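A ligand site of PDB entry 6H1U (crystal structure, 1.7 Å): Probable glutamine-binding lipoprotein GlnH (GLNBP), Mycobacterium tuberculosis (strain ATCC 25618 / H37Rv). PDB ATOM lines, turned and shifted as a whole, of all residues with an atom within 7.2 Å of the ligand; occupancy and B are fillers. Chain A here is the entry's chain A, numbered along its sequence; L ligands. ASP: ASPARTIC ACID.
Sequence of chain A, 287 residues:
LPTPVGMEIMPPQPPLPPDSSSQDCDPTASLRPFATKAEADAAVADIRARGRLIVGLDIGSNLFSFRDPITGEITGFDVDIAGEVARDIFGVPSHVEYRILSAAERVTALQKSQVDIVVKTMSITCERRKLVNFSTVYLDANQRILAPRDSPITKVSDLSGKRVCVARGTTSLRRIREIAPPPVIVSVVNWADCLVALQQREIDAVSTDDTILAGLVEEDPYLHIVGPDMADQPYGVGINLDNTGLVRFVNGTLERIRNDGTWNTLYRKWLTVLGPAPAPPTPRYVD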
ATOM      1  N   ALA A 103      16.196 -27.406 -15.356  1.00  0.00           N
ATOM      2  CA  ALA A 103      14.908 -27.910 -14.864  1.00  0.00           C
ATOM      3  C   ALA A 103      14.658 -29.334 -15.334  1.00  0.00           C
ATOM      4  O   ALA A 103      14.119 -30.167 -14.582  1.00  0.00           O
ATOM      5  CB  ALA A 103      13.780 -26.990 -15.332  1.00  0.00           C
ATOM      6  N   ARG A 106      16.455 -32.269 -13.117  1.00  0.00           N
ATOM      7  CA  ARG A 106      16.321 -32.367 -11.661  1.00  0.00           C
ATOM      8  C   ARG A 106      16.031 -33.805 -11.235  1.00  0.00           C
ATOM      9  O   ARG A 106      16.614 -34.292 -10.247  1.00  0.00           O
ATOM     10  CB  ARG A 106      15.223 -31.437 -11.163  1.00  0.00           C
ATOM     11  CG  ARG A 106      15.593 -29.957 -11.274  1.00  0.00           C
ATOM     12  CD  ARG A 106      14.416 -29.069 -10.888  1.00  0.00           C
ATOM     13  NE  ARG A 106      13.360 -29.116 -11.899  1.00  0.00           N
ATOM     14  CZ  ARG A 106      12.251 -28.370 -11.858  1.00  0.00           C
ATOM     15  NH1 ARG A 106      12.043 -27.543 -10.834  1.00  0.00           N
ATOM     16  NH2 ARG A 106      11.364 -28.451 -12.840  1.00  0.00           N
ATOM     17  N   LYS A 120      15.628 -26.476  -6.222  1.00  0.00           N
ATOM     18  CA  LYS A 120      15.517 -25.730  -7.480  1.00  0.00           C
ATOM     19  C   LYS A 120      14.027 -25.664  -7.828  1.00  0.00           C
ATOM     20  O   LYS A 120      13.562 -26.384  -8.718  1.00  0.00           O
ATOM     21  CB  LYS A 120      16.338 -26.355  -8.607  1.00  0.00           C
ATOM     22  CG  LYS A 120      16.530 -25.395  -9.779  1.00  0.00           C
ATOM     23  CD  LYS A 120      17.141 -26.083 -10.985  1.00  0.00           C
ATOM     24  CE  LYS A 120      17.471 -25.072 -12.062  1.00  0.00           C
ATOM     25  NZ  LYS A 120      16.393 -24.054 -12.225  1.00  0.00           N
ATOM     26  N   THR A 121      13.314 -24.792  -7.105  1.00  0.00           N
ATOM     27  CA  THR A 121      11.875 -24.504  -7.265  1.00  0.00           C
ATOM     28  C   THR A 121      11.093 -25.747  -7.681  1.00  0.00           C
ATOM     29  O   THR A 121      10.294 -25.685  -8.615  1.00  0.00           O
ATOM     30  CB  THR A 121      11.651 -23.350  -8.272  1.00  0.00           C
ATOM     31  OG1 THR A 121      12.192 -23.678  -9.566  1.00  0.00           O
ATOM     32  CG2 THR A 121      12.326 -22.068  -7.793  1.00  0.00           C
ATOM     33  N   MET A 122      11.275 -26.868  -6.986  1.00  0.00           N
ATOM     34  CA  MET A 122      10.828 -28.146  -7.536  1.00  0.00           C
ATOM     35  C   MET A 122       9.437 -28.493  -7.003  1.00  0.00           C
ATOM     36  O   MET A 122       9.285 -28.937  -5.869  1.00  0.00           O
ATOM     37  CB  MET A 122      11.859 -29.240  -7.225  1.00  0.00           C
ATOM     38  CG  MET A 122      11.645 -30.485  -8.060  1.00  0.00           C
ATOM     39  SD  MET A 122      12.982 -31.658  -7.793  1.00  0.00           S
ATOM     40  CE  MET A 122      12.517 -32.942  -8.948  1.00  0.00           C
ATOM     41  N   SER A 123       8.427 -28.323  -7.850  1.00  0.00           N
ATOM     42  CA  SER A 123       7.056 -28.635  -7.456  1.00  0.00           C
ATOM     43  C   SER A 123       6.903 -30.116  -7.167  1.00  0.00           C
ATOM     44  O   SER A 123       7.364 -30.957  -7.944  1.00  0.00           O
ATOM     45  CB  SER A 123       6.081 -28.219  -8.540  1.00  0.00           C
ATOM     46  OG  SER A 123       6.109 -26.814  -8.684  1.00  0.00           O
ATOM     47  N   ILE A 124       6.242 -30.412  -6.057  1.00  0.00           N
ATOM     48  CA  ILE A 124       5.943 -31.781  -5.639  1.00  0.00           C
ATOM     49  C   ILE A 124       4.699 -32.243  -6.379  1.00  0.00           C
ATOM     50  O   ILE A 124       3.614 -31.658  -6.217  1.00  0.00           O
ATOM     51  CB  ILE A 124       5.723 -31.853  -4.116  1.00  0.00           C
ATOM     52  CG1 ILE A 124       6.933 -31.302  -3.358  1.00  0.00           C
ATOM     53  CG2 ILE A 124       5.424 -33.279  -3.674  1.00  0.00           C
ATOM     54  CD1 ILE A 124       6.551 -30.798  -1.952  1.00  0.00           C
ATOM     55  N   THR A 125       4.830 -33.295  -7.187  1.00  0.00           N
ATOM     56  CA  THR A 125       3.705 -33.834  -7.943  1.00  0.00           C
ATOM     57  C   THR A 125       3.636 -35.346  -7.778  1.00  0.00           C
ATOM     58  O   THR A 125       4.628 -36.004  -7.466  1.00  0.00           O
ATOM     59  CB  THR A 125       3.806 -33.517  -9.440  1.00  0.00           C
ATOM     60  OG1 THR A 125       4.908 -34.232  -9.998  1.00  0.00           O
ATOM     61  CG2 THR A 125       4.003 -32.022  -9.672  1.00  0.00           C
ATOM     62  N   ARG A 128       6.054 -36.970 -10.240  1.00  0.00           N
ATOM     63  CA  ARG A 128       7.442 -36.961  -9.828  1.00  0.00           C
ATOM     64  C   ARG A 128       7.695 -37.882  -8.635  1.00  0.00           C
ATOM     65  O   ARG A 128       8.793 -38.429  -8.506  1.00  0.00           O
ATOM     66  CB  ARG A 128       7.885 -35.536  -9.501  1.00  0.00           C
ATOM     67  CG  ARG A 128       8.042 -34.707 -10.767  1.00  0.00           C
ATOM     68  CD  ARG A 128       8.281 -33.249 -10.421  1.00  0.00           C
ATOM     69  NE  ARG A 128       8.457 -32.462 -11.644  1.00  0.00           N
ATOM     70  CZ  ARG A 128       8.612 -31.137 -11.670  1.00  0.00           C
ATOM     71  NH1 ARG A 128       8.604 -30.451 -10.525  1.00  0.00           N
ATOM     72  NH2 ARG A 128       8.758 -30.498 -12.824  1.00  0.00           N
ATOM     73  N   ALA A 141       4.023 -21.646  -4.316  1.00  0.00           N
ATOM     74  CA  ALA A 141       3.850 -20.675  -5.403  1.00  0.00           C
ATOM     75  C   ALA A 141       2.618 -21.028  -6.230  1.00  0.00           C
ATOM     76  O   ALA A 141       1.937 -22.039  -5.983  1.00  0.00           O
ATOM     77  CB  ALA A 141       5.110 -20.604  -6.287  1.00  0.00           C
ATOM     78  N   ALA A 167      10.039 -23.166 -20.032  1.00  0.00           N
ATOM     79  CA  ALA A 167      11.262 -23.953 -19.921  1.00  0.00           C
ATOM     80  C   ALA A 167      10.931 -25.439 -19.987  1.00  0.00           C
ATOM     81  O   ALA A 167       9.946 -25.896 -19.401  1.00  0.00           O
ATOM     82  CB  ALA A 167      12.000 -23.640 -18.609  1.00  0.00           C
ATOM     83  N   ARG A 168      11.747 -26.196 -20.718  1.00  0.00           N
ATOM     84  CA  ARG A 168      11.522 -27.632 -20.797  1.00  0.00           C
ATOM     85  C   ARG A 168      11.704 -28.292 -19.435  1.00  0.00           C
ATOM     86  O   ARG A 168      12.514 -27.853 -18.611  1.00  0.00           O
ATOM     87  CB  ARG A 168      12.469 -28.255 -21.830  1.00  0.00           C
ATOM     88  CG  ARG A 168      12.089 -27.833 -23.256  1.00  0.00           C
ATOM     89  CD  ARG A 168      12.867 -28.565 -24.328  1.00  0.00           C
ATOM     90  NE  ARG A 168      14.246 -28.100 -24.445  1.00  0.00           N
ATOM     91  CZ  ARG A 168      14.598 -27.020 -25.138  1.00  0.00           C
ATOM     92  NH1 ARG A 168      13.671 -26.311 -25.752  1.00  0.00           N
ATOM     93  NH2 ARG A 168      15.880 -26.665 -25.223  1.00  0.00           N
ATOM     94  N   GLY A 169      10.943 -29.355 -19.212  1.00  0.00           N
ATOM     95  CA  GLY A 169      11.069 -30.085 -17.965  1.00  0.00           C
ATOM     96  C   GLY A 169      10.336 -29.459 -16.800  1.00  0.00           C
ATOM     97  O   GLY A 169      10.688 -29.752 -15.641  1.00  0.00           O
ATOM     98  N   THR A 170       9.331 -28.629 -17.046  1.00  0.00           N
ATOM     99  CA  THR A 170       8.626 -27.943 -15.966  1.00  0.00           C
ATOM    100  C   THR A 170       7.146 -28.327 -15.947  1.00  0.00           C
ATOM    101  O   THR A 170       6.581 -28.727 -16.961  1.00  0.00           O
ATOM    102  CB  THR A 170       8.744 -26.412 -16.067  1.00  0.00           C
ATOM    103  OG1 THR A 170       8.152 -25.966 -17.299  1.00  0.00           O
ATOM    104  CG2 THR A 170      10.207 -25.973 -16.013  1.00  0.00           C
ATOM    105  N   THR A 171       6.546 -28.212 -14.761  1.00  0.00           N
ATOM    106  CA  THR A 171       5.096 -28.368 -14.632  1.00  0.00           C
ATOM    107  C   THR A 171       4.358 -27.320 -15.434  1.00  0.00           C
ATOM    108  O   THR A 171       3.193 -27.519 -15.793  1.00  0.00           O
ATOM    109  CB  THR A 171       4.660 -28.229 -13.169  1.00  0.00           C
ATOM    110  OG1 THR A 171       5.090 -26.957 -12.661  1.00  0.00           O
ATOM    111  CG2 THR A 171       5.224 -29.373 -12.302  1.00  0.00           C
ATOM    112  N   SER A 172       5.013 -26.192 -15.691  1.00  0.00           N
ATOM    113  CA  SER A 172       4.366 -25.077 -16.363  1.00  0.00           C
ATOM    114  C   SER A 172       3.874 -25.476 -17.748  1.00  0.00           C
ATOM    115  O   SER A 172       2.826 -25.006 -18.202  1.00  0.00           O
ATOM    116  CB  SER A 172       5.338 -23.904 -16.462  1.00  0.00           C
ATOM    117  OG  SER A 172       5.935 -23.691 -15.192  1.00  0.00           O
ATOM    118  N   LEU A 173       4.625 -26.353 -18.427  1.00  0.00           N
ATOM    119  CA  LEU A 173       4.251 -26.808 -19.764  1.00  0.00           C
ATOM    120  C   LEU A 173       2.922 -27.550 -19.754  1.00  0.00           C
ATOM    121  O   LEU A 173       2.051 -27.301 -20.605  1.00  0.00           O
ATOM    122  CB  LEU A 173       5.349 -27.703 -20.349  1.00  0.00           C
ATOM    123  CG  LEU A 173       4.953 -28.403 -21.650  1.00  0.00           C
ATOM    124  CD1 LEU A 173       4.562 -27.358 -22.714  1.00  0.00           C
ATOM    125  CD2 LEU A 173       6.058 -29.313 -22.154  1.00  0.00           C
ATOM    126  N   ARG A 174       2.762 -28.493 -18.829  1.00  0.00           N
ATOM    127  CA  ARG A 174       1.524 -29.271 -18.728  1.00  0.00           C
ATOM    128  C   ARG A 174       0.307 -28.357 -18.665  1.00  0.00           C
ATOM    129  O   ARG A 174      -0.689 -28.568 -19.355  1.00  0.00           O
ATOM    130  CB  ARG A 174       1.582 -30.187 -17.503  1.00  0.00           C
ATOM    131  CG  ARG A 174       0.499 -31.237 -17.412  1.00  0.00           C
ATOM    132  CD  ARG A 174       0.964 -32.417 -16.530  1.00  0.00           C
ATOM    133  NE  ARG A 174       1.107 -32.092 -15.110  1.00  0.00           N
ATOM    134  CZ  ARG A 174       2.257 -31.775 -14.506  1.00  0.00           C
ATOM    135  NH1 ARG A 174       2.258 -31.507 -13.203  1.00  0.00           N
ATOM    136  NH2 ARG A 174       3.411 -31.721 -15.180  1.00  0.00           N
ATOM    137  N   TRP A 191      14.259 -20.277 -17.615  1.00  0.00           N
ATOM    138  CA  TRP A 191      13.324 -19.157 -17.614  1.00  0.00           C
ATOM    139  C   TRP A 191      14.016 -17.837 -17.963  1.00  0.00           C
ATOM    140  O   TRP A 191      13.375 -16.944 -18.533  1.00  0.00           O
ATOM    141  CB  TRP A 191      12.608 -19.059 -16.254  1.00  0.00           C
ATOM    142  CG  TRP A 191      11.696 -20.236 -16.040  1.00  0.00           C
ATOM    143  CD1 TRP A 191      11.874 -21.251 -15.132  1.00  0.00           C
ATOM    144  CD2 TRP A 191      10.501 -20.540 -16.766  1.00  0.00           C
ATOM    145  NE1 TRP A 191      10.841 -22.159 -15.235  1.00  0.00           N
ATOM    146  CE2 TRP A 191       9.992 -21.756 -16.231  1.00  0.00           C
ATOM    147  CE3 TRP A 191       9.804 -19.912 -17.802  1.00  0.00           C
ATOM    148  CZ2 TRP A 191       8.821 -22.346 -16.718  1.00  0.00           C
ATOM    149  CZ3 TRP A 191       8.637 -20.489 -18.271  1.00  0.00           C
ATOM    150  CH2 TRP A 191       8.155 -21.695 -17.723  1.00  0.00           C
ATOM    151  N   THR A 208       4.691 -19.210 -15.755  1.00  0.00           N
ATOM    152  CA  THR A 208       5.249 -20.139 -14.763  1.00  0.00           C
ATOM    153  C   THR A 208       4.931 -19.596 -13.369  1.00  0.00           C
ATOM    154  O   THR A 208       4.123 -18.685 -13.208  1.00  0.00           O
ATOM    155  CB  THR A 208       6.745 -20.362 -14.987  1.00  0.00           C
ATOM    156  OG1 THR A 208       7.218 -21.440 -14.153  1.00  0.00           O
ATOM    157  CG2 THR A 208       7.574 -19.115 -14.683  1.00  0.00           C
ATOM    158  N   ASP A 209       5.566 -20.207 -12.363  1.00  0.00           N
ATOM    159  CA  ASP A 209       5.395 -19.821 -10.958  1.00  0.00           C
ATOM    160  C   ASP A 209       5.523 -18.314 -10.786  1.00  0.00           C
ATOM    161  O   ASP A 209       6.486 -17.704 -11.283  1.00  0.00           O
ATOM    162  CB  ASP A 209       6.467 -20.479 -10.098  1.00  0.00           C
ATOM    163  CG  ASP A 209       6.576 -21.990 -10.281  1.00  0.00           C
ATOM    164  OD1 ASP A 209       5.802 -22.602 -11.036  1.00  0.00           O
ATOM    165  OD2 ASP A 209       7.473 -22.548  -9.632  1.00  0.00           O
ATOM    166  N   THR A 211       6.487 -16.736  -8.273  1.00  0.00           N
ATOM    167  CA  THR A 211       7.781 -16.519  -7.646  1.00  0.00           C
ATOM    168  C   THR A 211       8.894 -16.334  -8.686  1.00  0.00           C
ATOM    169  O   THR A 211       9.687 -15.387  -8.607  1.00  0.00           O
ATOM    170  CB  THR A 211       8.111 -17.725  -6.755  1.00  0.00           C
ATOM    171  OG1 THR A 211       7.823 -18.910  -7.511  1.00  0.00           O
ATOM    172  CG2 THR A 211       7.259 -17.711  -5.501  1.00  0.00           C
ATOM    173  N   ILE A 212       8.992 -17.267  -9.638  1.00  0.00           N
ATOM    174  CA  ILE A 212       9.964 -17.166 -10.714  1.00  0.00           C
ATOM    175  C   ILE A 212       9.699 -15.932 -11.564  1.00  0.00           C
ATOM    176  O   ILE A 212      10.623 -15.188 -11.928  1.00  0.00           O
ATOM    177  CB  ILE A 212       9.932 -18.449 -11.576  1.00  0.00           C
ATOM    178  CG1 ILE A 212      10.343 -19.664 -10.712  1.00  0.00           C
ATOM    179  CG2 ILE A 212      10.811 -18.293 -12.819  1.00  0.00           C
ATOM    180  CD1 ILE A 212      10.324 -20.965 -11.479  1.00  0.00           C
ATOM    181  N   GLN A 233       1.867 -24.716  -7.027  1.00  0.00           N
ATOM    182  CA  GLN A 233       3.259 -25.151  -7.189  1.00  0.00           C
ATOM    183  C   GLN A 233       3.909 -25.273  -5.816  1.00  0.00           C
ATOM    184  O   GLN A 233       4.594 -24.364  -5.353  1.00  0.00           O
ATOM    185  CB  GLN A 233       4.041 -24.176  -8.075  1.00  0.00           C
ATOM    186  CG  GLN A 233       3.356 -23.846  -9.402  1.00  0.00           C
ATOM    187  CD  GLN A 233       3.265 -25.047 -10.341  1.00  0.00           C
ATOM    188  OE1 GLN A 233       4.100 -25.941 -10.291  1.00  0.00           O
ATOM    189  NE2 GLN A 233       2.250 -25.057 -11.215  1.00  0.00           N
ATOM    190  N   PRO A 234       3.703 -26.397  -5.142  1.00  0.00           N
ATOM    191  CA  PRO A 234       4.273 -26.564  -3.800  1.00  0.00           C
ATOM    192  C   PRO A 234       5.701 -27.069  -3.870  1.00  0.00           C
ATOM    193  O   PRO A 234       5.931 -28.219  -4.267  1.00  0.00           O
ATOM    194  CB  PRO A 234       3.338 -27.578  -3.144  1.00  0.00           C
ATOM    195  CG  PRO A 234       2.863 -28.442  -4.300  1.00  0.00           C
ATOM    196  CD  PRO A 234       2.934 -27.575  -5.569  1.00  0.00           C
ATOM    197  N   TYR A 235       6.676 -26.235  -3.499  1.00  0.00           N
ATOM    198  CA  TYR A 235       8.072 -26.625  -3.649  1.00  0.00           C
ATOM    199  C   TYR A 235       8.510 -27.614  -2.576  1.00  0.00           C
ATOM    200  O   TYR A 235       8.228 -27.425  -1.394  1.00  0.00           O
ATOM    201  CB  TYR A 235       9.010 -25.434  -3.554  1.00  0.00           C
ATOM    202  CG  TYR A 235       8.898 -24.399  -4.635  1.00  0.00           C
ATOM    203  CD1 TYR A 235       8.061 -24.573  -5.727  1.00  0.00           C
ATOM    204  CD2 TYR A 235       9.638 -23.224  -4.554  1.00  0.00           C
ATOM    205  CE1 TYR A 235       7.978 -23.581  -6.730  1.00  0.00           C
ATOM    206  CE2 TYR A 235       9.555 -22.248  -5.544  1.00  0.00           C
ATOM    207  CZ  TYR A 235       8.724 -22.434  -6.618  1.00  0.00           C
ATOM    208  OH  TYR A 235       8.653 -21.449  -7.596  1.00  0.00           O
HETATM  209  N   ASP L   1       8.087 -25.160 -10.080  1.00  0.00           N
HETATM  210  CA  ASP L   1       7.872 -25.576 -11.460  1.00  0.00           C
HETATM  211  C   ASP L   1       8.401 -26.986 -11.689  1.00  0.00           C
HETATM  212  O   ASP L   1       8.533 -27.434 -12.825  1.00  0.00           O
HETATM  213  CB  ASP L   1       8.549 -24.582 -12.444  1.00  0.00           C
HETATM  214  CG  ASP L   1      10.065 -24.628 -12.372  1.00  0.00           C
HETATM  215  OD1 ASP L   1      10.721 -24.058 -13.260  1.00  0.00           O
HETATM  216  OD2 ASP L   1      10.613 -25.223 -11.415  1.00  0.00           O
HETATM  217  OXT ASP L   1       8.707 -27.671 -10.698  1.00  0.00           O
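The backbone carbonyl oxygen (O) of Thr 121 is in hydrogen-bond range of a nitrogen (N) of the ligand, 2.7 Å away.
An oxygen (OD2) of the ligand is in hydrogen-bond range of the side-chain hydroxyl (OG1) of Thr 121 (2.9 Å).
The side-chain carboxylate (OD2) of Asp 209 is in salt-bridge range of a nitrogen (N) of the ligand, at 2.7 Å.
OD1 of the ligand sits at hydrogen-bond distance from NE1 of Trp 191, at 2.7 Å.
The guanidinium group (NH1) of Arg 128 is in salt-bridge range of an oxygen (OXT) of the ligand, at 2.8 Å.
An oxygen (OD2) of the ligand lies within salt-bridge range of the guanidinium group (NH1) of Arg 106, 2.8 Å away.
The backbone NH (N) of Thr 171 sits at hydrogen-bond distance from an oxygen (O) of the ligand (2.9 Å).
An oxygen (O) of the ligand sits close to the side-chain hydroxyl of Thr 171 (3.5 Å).
N of Ser 123 is in hydrogen-bond range of OXT of the ligand (2.9 Å).
N of the ligand is in hydrogen-bond range of OG of Ser 123 (2.9 Å).
OD2 of Asp 209 is in hydrogen-bond range of OH of Tyr 235 (2.6 Å).
The guanidinium group (NH1) of Arg 128 is in hydrogen-bond range of the backbone carbonyl oxygen (O) of Ser 123, at 2.9 Å.
The guanidinium group (NH2) of Arg 128 is in hydrogen-bond range of the backbone carbonyl oxygen (O) of Gly 169 (3.5 Å).
The backbone NH (N) of Arg 128 lies within hydrogen-bond range of the side-chain hydroxyl (OG1) of Thr 125, 3.0 Å away.
NH2 of Arg 106 sits at hydrogen-bond distance from O of Gly 169 (3.2 Å).
OG1 of Thr 170 lies within hydrogen-bond range of O of Ala 167 (2.8 Å).
OH of Tyr 235 is in hydrogen-bond range of OG1 of Thr 211, 2.7 Å away.
OG1 of Thr 208 sits at hydrogen-bond distance from OG of Ser 172, 2.8 Å away.
Met 122 touches the ligand.
CA of Thr 170 touches O of the ligand, at 3.2 Å.
Ser 172 touches the ligand.
Thr 208 touches the ligand.
Ile 212 touches the ligand (CD1 to OD1, 3.6 Å).
OE1 of Gln 233 touches CA of the ligand (3.97 Å).
CE1 of Tyr 235 touches N of the ligand, at 3.7 Å.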
